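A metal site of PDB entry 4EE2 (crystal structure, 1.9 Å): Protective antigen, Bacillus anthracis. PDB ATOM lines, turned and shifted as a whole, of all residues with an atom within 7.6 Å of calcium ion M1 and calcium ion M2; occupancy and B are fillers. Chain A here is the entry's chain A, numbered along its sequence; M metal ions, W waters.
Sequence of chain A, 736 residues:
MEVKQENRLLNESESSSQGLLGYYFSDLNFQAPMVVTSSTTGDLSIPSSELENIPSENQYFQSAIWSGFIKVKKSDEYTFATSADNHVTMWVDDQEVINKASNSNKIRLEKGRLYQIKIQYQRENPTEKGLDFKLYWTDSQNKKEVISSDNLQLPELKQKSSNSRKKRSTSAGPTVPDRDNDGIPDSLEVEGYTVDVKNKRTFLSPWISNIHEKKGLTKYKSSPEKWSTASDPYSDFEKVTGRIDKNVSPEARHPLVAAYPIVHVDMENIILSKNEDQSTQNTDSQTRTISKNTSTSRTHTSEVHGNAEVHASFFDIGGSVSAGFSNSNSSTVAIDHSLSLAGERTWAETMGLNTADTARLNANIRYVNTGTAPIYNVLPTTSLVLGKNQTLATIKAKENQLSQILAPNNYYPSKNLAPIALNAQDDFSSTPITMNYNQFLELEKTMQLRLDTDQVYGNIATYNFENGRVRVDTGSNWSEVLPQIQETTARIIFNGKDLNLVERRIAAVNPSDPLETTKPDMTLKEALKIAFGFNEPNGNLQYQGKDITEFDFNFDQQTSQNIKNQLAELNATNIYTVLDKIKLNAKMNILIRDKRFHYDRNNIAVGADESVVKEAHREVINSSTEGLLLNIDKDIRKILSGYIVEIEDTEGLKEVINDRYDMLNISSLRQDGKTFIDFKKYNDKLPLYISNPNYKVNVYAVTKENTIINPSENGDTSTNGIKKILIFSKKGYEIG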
ATOM      1  N   TYR A  23      40.865  18.703  31.335  1.00  0.00           N
ATOM      2  CA  TYR A  23      40.351  19.529  30.250  1.00  0.00           C
ATOM      3  C   TYR A  23      41.222  20.772  30.110  1.00  0.00           C
ATOM      4  O   TYR A  23      41.298  21.561  31.034  1.00  0.00           O
ATOM      5  CB  TYR A  23      38.913  19.976  30.533  1.00  0.00           C
ATOM      6  CG  TYR A  23      37.934  18.831  30.638  1.00  0.00           C
ATOM      7  CD1 TYR A  23      37.481  18.389  31.871  1.00  0.00           C
ATOM      8  CD2 TYR A  23      37.487  18.167  29.501  1.00  0.00           C
ATOM      9  CE1 TYR A  23      36.580  17.334  31.972  1.00  0.00           C
ATOM     10  CE2 TYR A  23      36.598  17.128  29.587  1.00  0.00           C
ATOM     11  CZ  TYR A  23      36.145  16.718  30.819  1.00  0.00           C
ATOM     12  OH  TYR A  23      35.258  15.675  30.883  1.00  0.00           O
ATOM     13  N   PRO A 177      31.107  21.142  30.639  1.00  0.00           N
ATOM     14  CA  PRO A 177      29.836  20.866  29.973  1.00  0.00           C
ATOM     15  C   PRO A 177      29.842  19.454  29.421  1.00  0.00           C
ATOM     16  O   PRO A 177      30.337  19.207  28.324  1.00  0.00           O
ATOM     17  CB  PRO A 177      29.807  21.887  28.837  1.00  0.00           C
ATOM     18  CG  PRO A 177      30.610  23.018  29.350  1.00  0.00           C
ATOM     19  CD  PRO A 177      31.702  22.420  30.194  1.00  0.00           C
ATOM     20  N   ASP A 178      29.268  18.538  30.195  1.00  0.00           N
ATOM     21  CA  ASP A 178      29.156  17.150  29.774  1.00  0.00           C
ATOM     22  C   ASP A 178      27.749  16.644  30.096  1.00  0.00           C
ATOM     23  O   ASP A 178      27.574  15.861  31.031  1.00  0.00           O
ATOM     24  CB  ASP A 178      30.197  16.311  30.504  1.00  0.00           C
ATOM     25  CG  ASP A 178      30.326  14.914  29.929  1.00  0.00           C
ATOM     26  OD1 ASP A 178      29.794  14.676  28.822  1.00  0.00           O
ATOM     27  OD2 ASP A 178      30.965  14.063  30.577  1.00  0.00           O
ATOM     28  N   ARG A 179      26.750  17.104  29.346  1.00  0.00           N
ATOM     29  CA  ARG A 179      25.366  16.718  29.625  1.00  0.00           C
ATOM     30  C   ARG A 179      25.147  15.208  29.850  1.00  0.00           C
ATOM     31  O   ARG A 179      24.339  14.822  30.690  1.00  0.00           O
ATOM     32  CB  ARG A 179      24.454  17.251  28.486  1.00  0.00           C
ATOM     33  CG  ARG A 179      24.423  18.777  28.395  1.00  0.00           C
ATOM     34  CD  ARG A 179      23.812  19.327  27.096  1.00  0.00           C
ATOM     35  NE  ARG A 179      22.346  19.392  27.117  1.00  0.00           N
ATOM     36  CZ  ARG A 179      21.649  20.340  27.738  1.00  0.00           C
ATOM     37  NH1 ARG A 179      22.275  21.293  28.418  1.00  0.00           N
ATOM     38  NH2 ARG A 179      20.325  20.319  27.696  1.00  0.00           N
ATOM     39  N   ASP A 180      25.874  14.344  29.132  1.00  0.00           N
ATOM     40  CA  ASP A 180      25.627  12.898  29.247  1.00  0.00           C
ATOM     41  C   ASP A 180      26.626  12.162  30.142  1.00  0.00           C
ATOM     42  O   ASP A 180      26.524  10.952  30.338  1.00  0.00           O
ATOM     43  CB  ASP A 180      25.563  12.239  27.871  1.00  0.00           C
ATOM     44  CG  ASP A 180      26.798  12.528  27.028  1.00  0.00           C
ATOM     45  OD1 ASP A 180      27.817  12.991  27.576  1.00  0.00           O
ATOM     46  OD2 ASP A 180      26.733  12.268  25.819  1.00  0.00           O
ATOM     47  N   ASN A 181      27.577  12.909  30.678  1.00  0.00           N
ATOM     48  CA  ASN A 181      28.554  12.376  31.623  1.00  0.00           C
ATOM     49  C   ASN A 181      29.445  11.291  31.013  1.00  0.00           C
ATOM     50  O   ASN A 181      29.945  10.432  31.727  1.00  0.00           O
ATOM     51  CB  ASN A 181      27.876  11.841  32.906  1.00  0.00           C
ATOM     52  CG  ASN A 181      28.855  11.671  34.073  1.00  0.00           C
ATOM     53  OD1 ASN A 181      28.753  10.738  34.863  1.00  0.00           O
ATOM     54  ND2 ASN A 181      29.816  12.573  34.173  1.00  0.00           N
ATOM     55  N   ASP A 182      29.685  11.344  29.707  1.00  0.00           N
ATOM     56  CA  ASP A 182      30.627  10.381  29.151  1.00  0.00           C
ATOM     57  C   ASP A 182      32.074  10.846  29.243  1.00  0.00           C
ATOM     58  O   ASP A 182      32.996  10.025  29.142  1.00  0.00           O
ATOM     59  CB  ASP A 182      30.240   9.935  27.731  1.00  0.00           C
ATOM     60  CG  ASP A 182      30.169  11.087  26.737  1.00  0.00           C
ATOM     61  OD1 ASP A 182      30.767  12.157  26.965  1.00  0.00           O
ATOM     62  OD2 ASP A 182      29.538  10.876  25.690  1.00  0.00           O
ATOM     63  N   GLY A 183      32.272  12.140  29.475  1.00  0.00           N
ATOM     64  CA  GLY A 183      33.611  12.698  29.615  1.00  0.00           C
ATOM     65  C   GLY A 183      34.036  13.629  28.492  1.00  0.00           C
ATOM     66  O   GLY A 183      34.963  14.427  28.650  1.00  0.00           O
ATOM     67  N   ILE A 184      33.363  13.539  27.352  1.00  0.00           N
ATOM     68  CA  ILE A 184      33.636  14.444  26.245  1.00  0.00           C
ATOM     69  C   ILE A 184      32.721  15.645  26.373  1.00  0.00           C
ATOM     70  O   ILE A 184      31.509  15.486  26.426  1.00  0.00           O
ATOM     71  CB  ILE A 184      33.379  13.777  24.886  1.00  0.00           C
ATOM     72  CG1 ILE A 184      33.965  12.355  24.862  1.00  0.00           C
ATOM     73  CG2 ILE A 184      33.959  14.626  23.755  1.00  0.00           C
ATOM     74  CD1 ILE A 184      33.657  11.591  23.604  1.00  0.00           C
ATOM     75  N   PRO A 185      33.306  16.850  26.431  1.00  0.00           N
ATOM     76  CA  PRO A 185      32.571  18.111  26.471  1.00  0.00           C
ATOM     77  C   PRO A 185      31.502  18.196  25.394  1.00  0.00           C
ATOM     78  O   PRO A 185      31.753  17.762  24.272  1.00  0.00           O
ATOM     79  CB  PRO A 185      33.665  19.148  26.197  1.00  0.00           C
ATOM     80  CG  PRO A 185      34.900  18.536  26.778  1.00  0.00           C
ATOM     81  CD  PRO A 185      34.766  17.053  26.557  1.00  0.00           C
ATOM     82  N   ASP A 186      30.338  18.765  25.715  1.00  0.00           N
ATOM     83  CA  ASP A 186      29.235  18.898  24.744  1.00  0.00           C
ATOM     84  C   ASP A 186      29.728  19.440  23.400  1.00  0.00           C
ATOM     85  O   ASP A 186      29.369  18.926  22.342  1.00  0.00           O
ATOM     86  CB  ASP A 186      28.167  19.876  25.258  1.00  0.00           C
ATOM     87  CG  ASP A 186      27.579  19.477  26.594  1.00  0.00           C
ATOM     88  OD1 ASP A 186      27.710  18.305  27.019  1.00  0.00           O
ATOM     89  OD2 ASP A 186      26.952  20.348  27.241  1.00  0.00           O
ATOM     90  N   SER A 187      30.529  20.502  23.459  1.00  0.00           N
ATOM     91  CA  SER A 187      30.899  21.234  22.256  1.00  0.00           C
ATOM     92  C   SER A 187      31.764  20.407  21.313  1.00  0.00           C
ATOM     93  O   SER A 187      31.648  20.522  20.101  1.00  0.00           O
ATOM     94  CB  SER A 187      31.595  22.565  22.609  1.00  0.00           C
ATOM     95  OG  SER A 187      32.844  22.346  23.242  1.00  0.00           O
ATOM     96  N   GLU A 189      31.745  16.963  21.085  1.00  0.00           N
ATOM     97  CA  GLU A 189      30.915  15.933  20.443  1.00  0.00           C
ATOM     98  C   GLU A 189      30.137  16.497  19.266  1.00  0.00           C
ATOM     99  O   GLU A 189      29.980  15.852  18.231  1.00  0.00           O
ATOM    100  CB  GLU A 189      29.951  15.296  21.450  1.00  0.00           C
ATOM    101  CG  GLU A 189      30.642  14.529  22.552  1.00  0.00           C
ATOM    102  CD  GLU A 189      29.728  13.524  23.237  1.00  0.00           C
ATOM    103  OE1 GLU A 189      29.382  12.515  22.593  1.00  0.00           O
ATOM    104  OE2 GLU A 189      29.356  13.769  24.401  1.00  0.00           O
ATOM    105  N   TYR A 193      35.601  15.875  16.699  1.00  0.00           N
ATOM    106  CA  TYR A 193      36.848  15.693  17.418  1.00  0.00           C
ATOM    107  C   TYR A 193      37.680  14.572  16.810  1.00  0.00           C
ATOM    108  O   TYR A 193      37.191  13.734  16.057  1.00  0.00           O
ATOM    109  CB  TYR A 193      36.582  15.428  18.897  1.00  0.00           C
ATOM    110  CG  TYR A 193      35.668  14.254  19.212  1.00  0.00           C
ATOM    111  CD1 TYR A 193      34.282  14.395  19.140  1.00  0.00           C
ATOM    112  CD2 TYR A 193      36.177  13.022  19.608  1.00  0.00           C
ATOM    113  CE1 TYR A 193      33.428  13.324  19.441  1.00  0.00           C
ATOM    114  CE2 TYR A 193      35.342  11.960  19.915  1.00  0.00           C
ATOM    115  CZ  TYR A 193      33.967  12.117  19.828  1.00  0.00           C
ATOM    116  OH  TYR A 193      33.124  11.061  20.114  1.00  0.00           O
ATOM    117  N   SER A 222      29.552  12.864  17.869  1.00  0.00           N
ATOM    118  CA  SER A 222      28.650  12.035  18.664  1.00  0.00           C
ATOM    119  C   SER A 222      27.560  12.900  19.298  1.00  0.00           C
ATOM    120  O   SER A 222      27.619  14.127  19.208  1.00  0.00           O
ATOM    121  CB  SER A 222      29.439  11.237  19.716  1.00  0.00           C
ATOM    122  OG  SER A 222      30.532  11.980  20.256  1.00  0.00           O
ATOM    123  N   SER A 223      26.563  12.287  19.918  1.00  0.00           N
ATOM    124  CA  SER A 223      25.565  13.077  20.645  1.00  0.00           C
ATOM    125  C   SER A 223      26.082  13.513  21.992  1.00  0.00           C
ATOM    126  O   SER A 223      26.573  12.708  22.765  1.00  0.00           O
ATOM    127  CB  SER A 223      24.258  12.325  20.869  1.00  0.00           C
ATOM    128  OG  SER A 223      23.415  13.084  21.730  1.00  0.00           O
ATOM    129  N   PRO A 224      25.968  14.813  22.306  1.00  0.00           N
ATOM    130  CA  PRO A 224      26.335  15.264  23.641  1.00  0.00           C
ATOM    131  C   PRO A 224      25.308  14.858  24.703  1.00  0.00           C
ATOM    132  O   PRO A 224      25.509  15.105  25.881  1.00  0.00           O
ATOM    133  CB  PRO A 224      26.383  16.793  23.487  1.00  0.00           C
ATOM    134  CG  PRO A 224      25.421  17.089  22.394  1.00  0.00           C
ATOM    135  CD  PRO A 224      25.562  15.928  21.431  1.00  0.00           C
ATOM    136  N   GLU A 225      24.207  14.243  24.287  1.00  0.00           N
ATOM    137  CA  GLU A 225      23.135  13.878  25.209  1.00  0.00           C
ATOM    138  C   GLU A 225      22.935  12.350  25.294  1.00  0.00           C
ATOM    139  O   GLU A 225      22.056  11.858  25.987  1.00  0.00           O
ATOM    140  CB  GLU A 225      21.863  14.607  24.819  1.00  0.00           C
ATOM    141  CG  GLU A 225      22.042  16.132  24.911  1.00  0.00           C
ATOM    142  CD  GLU A 225      20.764  16.935  24.723  1.00  0.00           C
ATOM    143  OE1 GLU A 225      19.660  16.343  24.810  1.00  0.00           O
ATOM    144  OE2 GLU A 225      20.872  18.163  24.470  1.00  0.00           O
ATOM    145  N   LYS A 226      23.769  11.619  24.578  1.00  0.00           N
ATOM    146  CA  LYS A 226      23.761  10.164  24.633  1.00  0.00           C
ATOM    147  C   LYS A 226      25.116   9.673  25.119  1.00  0.00           C
ATOM    148  O   LYS A 226      26.125   9.829  24.419  1.00  0.00           O
ATOM    149  CB  LYS A 226      23.412   9.555  23.272  1.00  0.00           C
ATOM    150  CG  LYS A 226      21.999   9.925  22.794  1.00  0.00           C
ATOM    151  CD  LYS A 226      21.650   9.341  21.419  1.00  0.00           C
ATOM    152  CE  LYS A 226      21.517   7.814  21.448  1.00  0.00           C
ATOM    153  NZ  LYS A 226      20.327   7.375  22.207  1.00  0.00           N
ATOM    154  N   TRP A 227      25.127   9.086  26.306  1.00  0.00           N
ATOM    155  CA  TRP A 227      26.345   8.556  26.922  1.00  0.00           C
ATOM    156  C   TRP A 227      27.007   7.560  25.944  1.00  0.00           C
ATOM    157  O   TRP A 227      28.223   7.604  25.717  1.00  0.00           O
ATOM    158  CB  TRP A 227      25.993   7.945  28.281  1.00  0.00           C
ATOM    159  CG  TRP A 227      27.103   7.231  28.995  1.00  0.00           C
ATOM    160  CD1 TRP A 227      28.020   7.768  29.861  1.00  0.00           C
ATOM    161  CD2 TRP A 227      27.379   5.826  28.951  1.00  0.00           C
ATOM    162  NE1 TRP A 227      28.855   6.786  30.332  1.00  0.00           N
ATOM    163  CE2 TRP A 227      28.480   5.583  29.802  1.00  0.00           C
ATOM    164  CE3 TRP A 227      26.807   4.741  28.268  1.00  0.00           C
ATOM    165  CZ2 TRP A 227      29.025   4.300  29.997  1.00  0.00           C
ATOM    166  CZ3 TRP A 227      27.353   3.471  28.456  1.00  0.00           C
ATOM    167  CH2 TRP A 227      28.453   3.259  29.307  1.00  0.00           C
ATOM    168  N   SER A 228      26.195   6.689  25.364  1.00  0.00           N
ATOM    169  CA  SER A 228      26.593   5.913  24.193  1.00  0.00           C
ATOM    170  C   SER A 228      25.716   6.339  23.035  1.00  0.00           C
ATOM    171  O   SER A 228      24.497   6.177  23.065  1.00  0.00           O
ATOM    172  CB  SER A 228      26.413   4.401  24.433  1.00  0.00           C
ATOM    173  OG  SER A 228      26.562   3.675  23.218  1.00  0.00           O
ATOM    174  N   THR A 229      26.312   6.909  21.997  1.00  0.00           N
ATOM    175  CA  THR A 229      25.515   7.434  20.911  1.00  0.00           C
ATOM    176  C   THR A 229      24.806   6.343  20.115  1.00  0.00           C
ATOM    177  O   THR A 229      23.717   6.562  19.584  1.00  0.00           O
ATOM    178  CB  THR A 229      26.346   8.385  20.009  1.00  0.00           C
ATOM    179  OG1 THR A 229      26.604   9.587  20.757  1.00  0.00           O
ATOM    180  CG2 THR A 229      25.571   8.759  18.772  1.00  0.00           C
ATOM    181  N   SER A 235      30.545   3.676  26.397  1.00  0.00           N
ATOM    182  CA  SER A 235      30.390   5.114  26.191  1.00  0.00           C
ATOM    183  C   SER A 235      31.224   5.643  25.030  1.00  0.00           C
ATOM    184  O   SER A 235      32.224   5.049  24.651  1.00  0.00           O
ATOM    185  CB  SER A 235      30.735   5.886  27.467  1.00  0.00           C
ATOM    186  OG  SER A 235      32.068   6.373  27.426  1.00  0.00           O
ATOM    187  N   ASP A 236      30.806   6.789  24.490  1.00  0.00           N
ATOM    188  CA  ASP A 236      31.521   7.411  23.376  1.00  0.00           C
ATOM    189  C   ASP A 236      32.990   7.641  23.754  1.00  0.00           C
ATOM    190  O   ASP A 236      33.890   7.489  22.944  1.00  0.00           O
ATOM    191  CB  ASP A 236      30.855   8.750  23.006  1.00  0.00           C
ATOM    192  CG  ASP A 236      29.405   8.591  22.536  1.00  0.00           C
ATOM    193  OD1 ASP A 236      29.034   7.508  22.024  1.00  0.00           O
ATOM    194  OD2 ASP A 236      28.619   9.552  22.654  1.00  0.00           O
ATOM    195  N   PHE A 237      33.207   8.033  25.011  1.00  0.00           N
ATOM    196  CA  PHE A 237      34.547   8.273  25.536  1.00  0.00           C
ATOM    197  C   PHE A 237      35.336   6.977  25.723  1.00  0.00           C
ATOM    198  O   PHE A 237      36.526   6.911  25.406  1.00  0.00           O
ATOM    199  CB  PHE A 237      34.433   8.996  26.871  1.00  0.00           C
ATOM    200  CG  PHE A 237      35.756   9.380  27.503  1.00  0.00           C
ATOM    201  CD1 PHE A 237      36.450  10.516  27.098  1.00  0.00           C
ATOM    202  CD2 PHE A 237      36.272   8.639  28.551  1.00  0.00           C
ATOM    203  CE1 PHE A 237      37.656  10.880  27.700  1.00  0.00           C
ATOM    204  CE2 PHE A 237      37.477   8.991  29.160  1.00  0.00           C
ATOM    205  CZ  PHE A 237      38.165  10.101  28.735  1.00  0.00           C
ATOM    206  N   PRO A 255      32.050   5.939  17.864  1.00  0.00           N
ATOM    207  CA  PRO A 255      30.847   6.239  18.643  1.00  0.00           C
ATOM    208  C   PRO A 255      29.550   6.067  17.839  1.00  0.00           C
ATOM    209  O   PRO A 255      28.482   5.907  18.436  1.00  0.00           O
ATOM    210  CB  PRO A 255      31.039   7.710  19.047  1.00  0.00           C
ATOM    211  CG  PRO A 255      32.535   7.850  19.147  1.00  0.00           C
ATOM    212  CD  PRO A 255      33.097   6.956  18.053  1.00  0.00           C
HETATM  213 CA    CA M   1      27.971  11.346  24.076  1.00  0.00          CA
HETATM  214 CA    CA M   2      29.587  14.213  26.678  1.00  0.00          CA
HETATM  215  O   HOH W   1      28.295  15.789  26.428  1.00  0.00           O
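OG1 of Thr 229 touches calcium ion M1, at 3.997 Å.
Seven residues have an atom within 4 Å of calcium ion M1: Asp 180, Asp 182, Glu 189, Ser 223, Lys 226, Thr 229 and Asp 236.
The nearest printed residue that does not touch calcium ion M1 is Trp 227 (4.1 Å).
O of Glu 189 is in hydrogen-bond range of N of Ser 222.
The side-chain carboxylate of Asp 178 sits close to the backbone NH of Asn 181 (3.4 Å).
OD1 of Asp 236 lies within hydrogen-bond range of N of Thr 229 (2.8 Å).
The backbone NH (N) of Ser 223 sits at hydrogen-bond distance from the side-chain hydroxyl (OG1) of Thr 229, at 2.8 Å.
The backbone NH (N) of Asp 236 is in hydrogen-bond range of the backbone carbonyl oxygen (O) of Trp 227 (3.0 Å).
The side-chain hydroxyl of Ser 223 sits at hydrogen-bond distance from the backbone NH of Lys 226, 3.2 Å away.
OD2 of Asp 178 lies within hydrogen-bond range of N of Gly 183 (2.6 Å).
The backbone NH of Asp 180 sits close to the backbone carbonyl oxygen of Pro 224, 3.4 Å away.
Of the 26 residues printed, 5 come within 4 Å of calcium ion M2.
Water W1 bridges OD1 of Asp 186 (2.6 Å) and O of Pro 224 (2.9 Å).
Calcium ion M2 is bound by water W1 (2.1 Å), OD1 of Asp 178 (2.2 Å), O of Ile 184 (2.3 Å), OD1 of Asp 180 (2.3 Å), OE2 of Glu 189 (2.3 Å) and OD1 of Asp 182 (2.4 Å).
Calcium ion M1 is bound by OD2 of Asp 182, OD2 of Asp 180, O of Ser 223, OE1 of Glu 189, OD2 of Asp 236, O of Lys 226 and OE2 of Glu 189.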
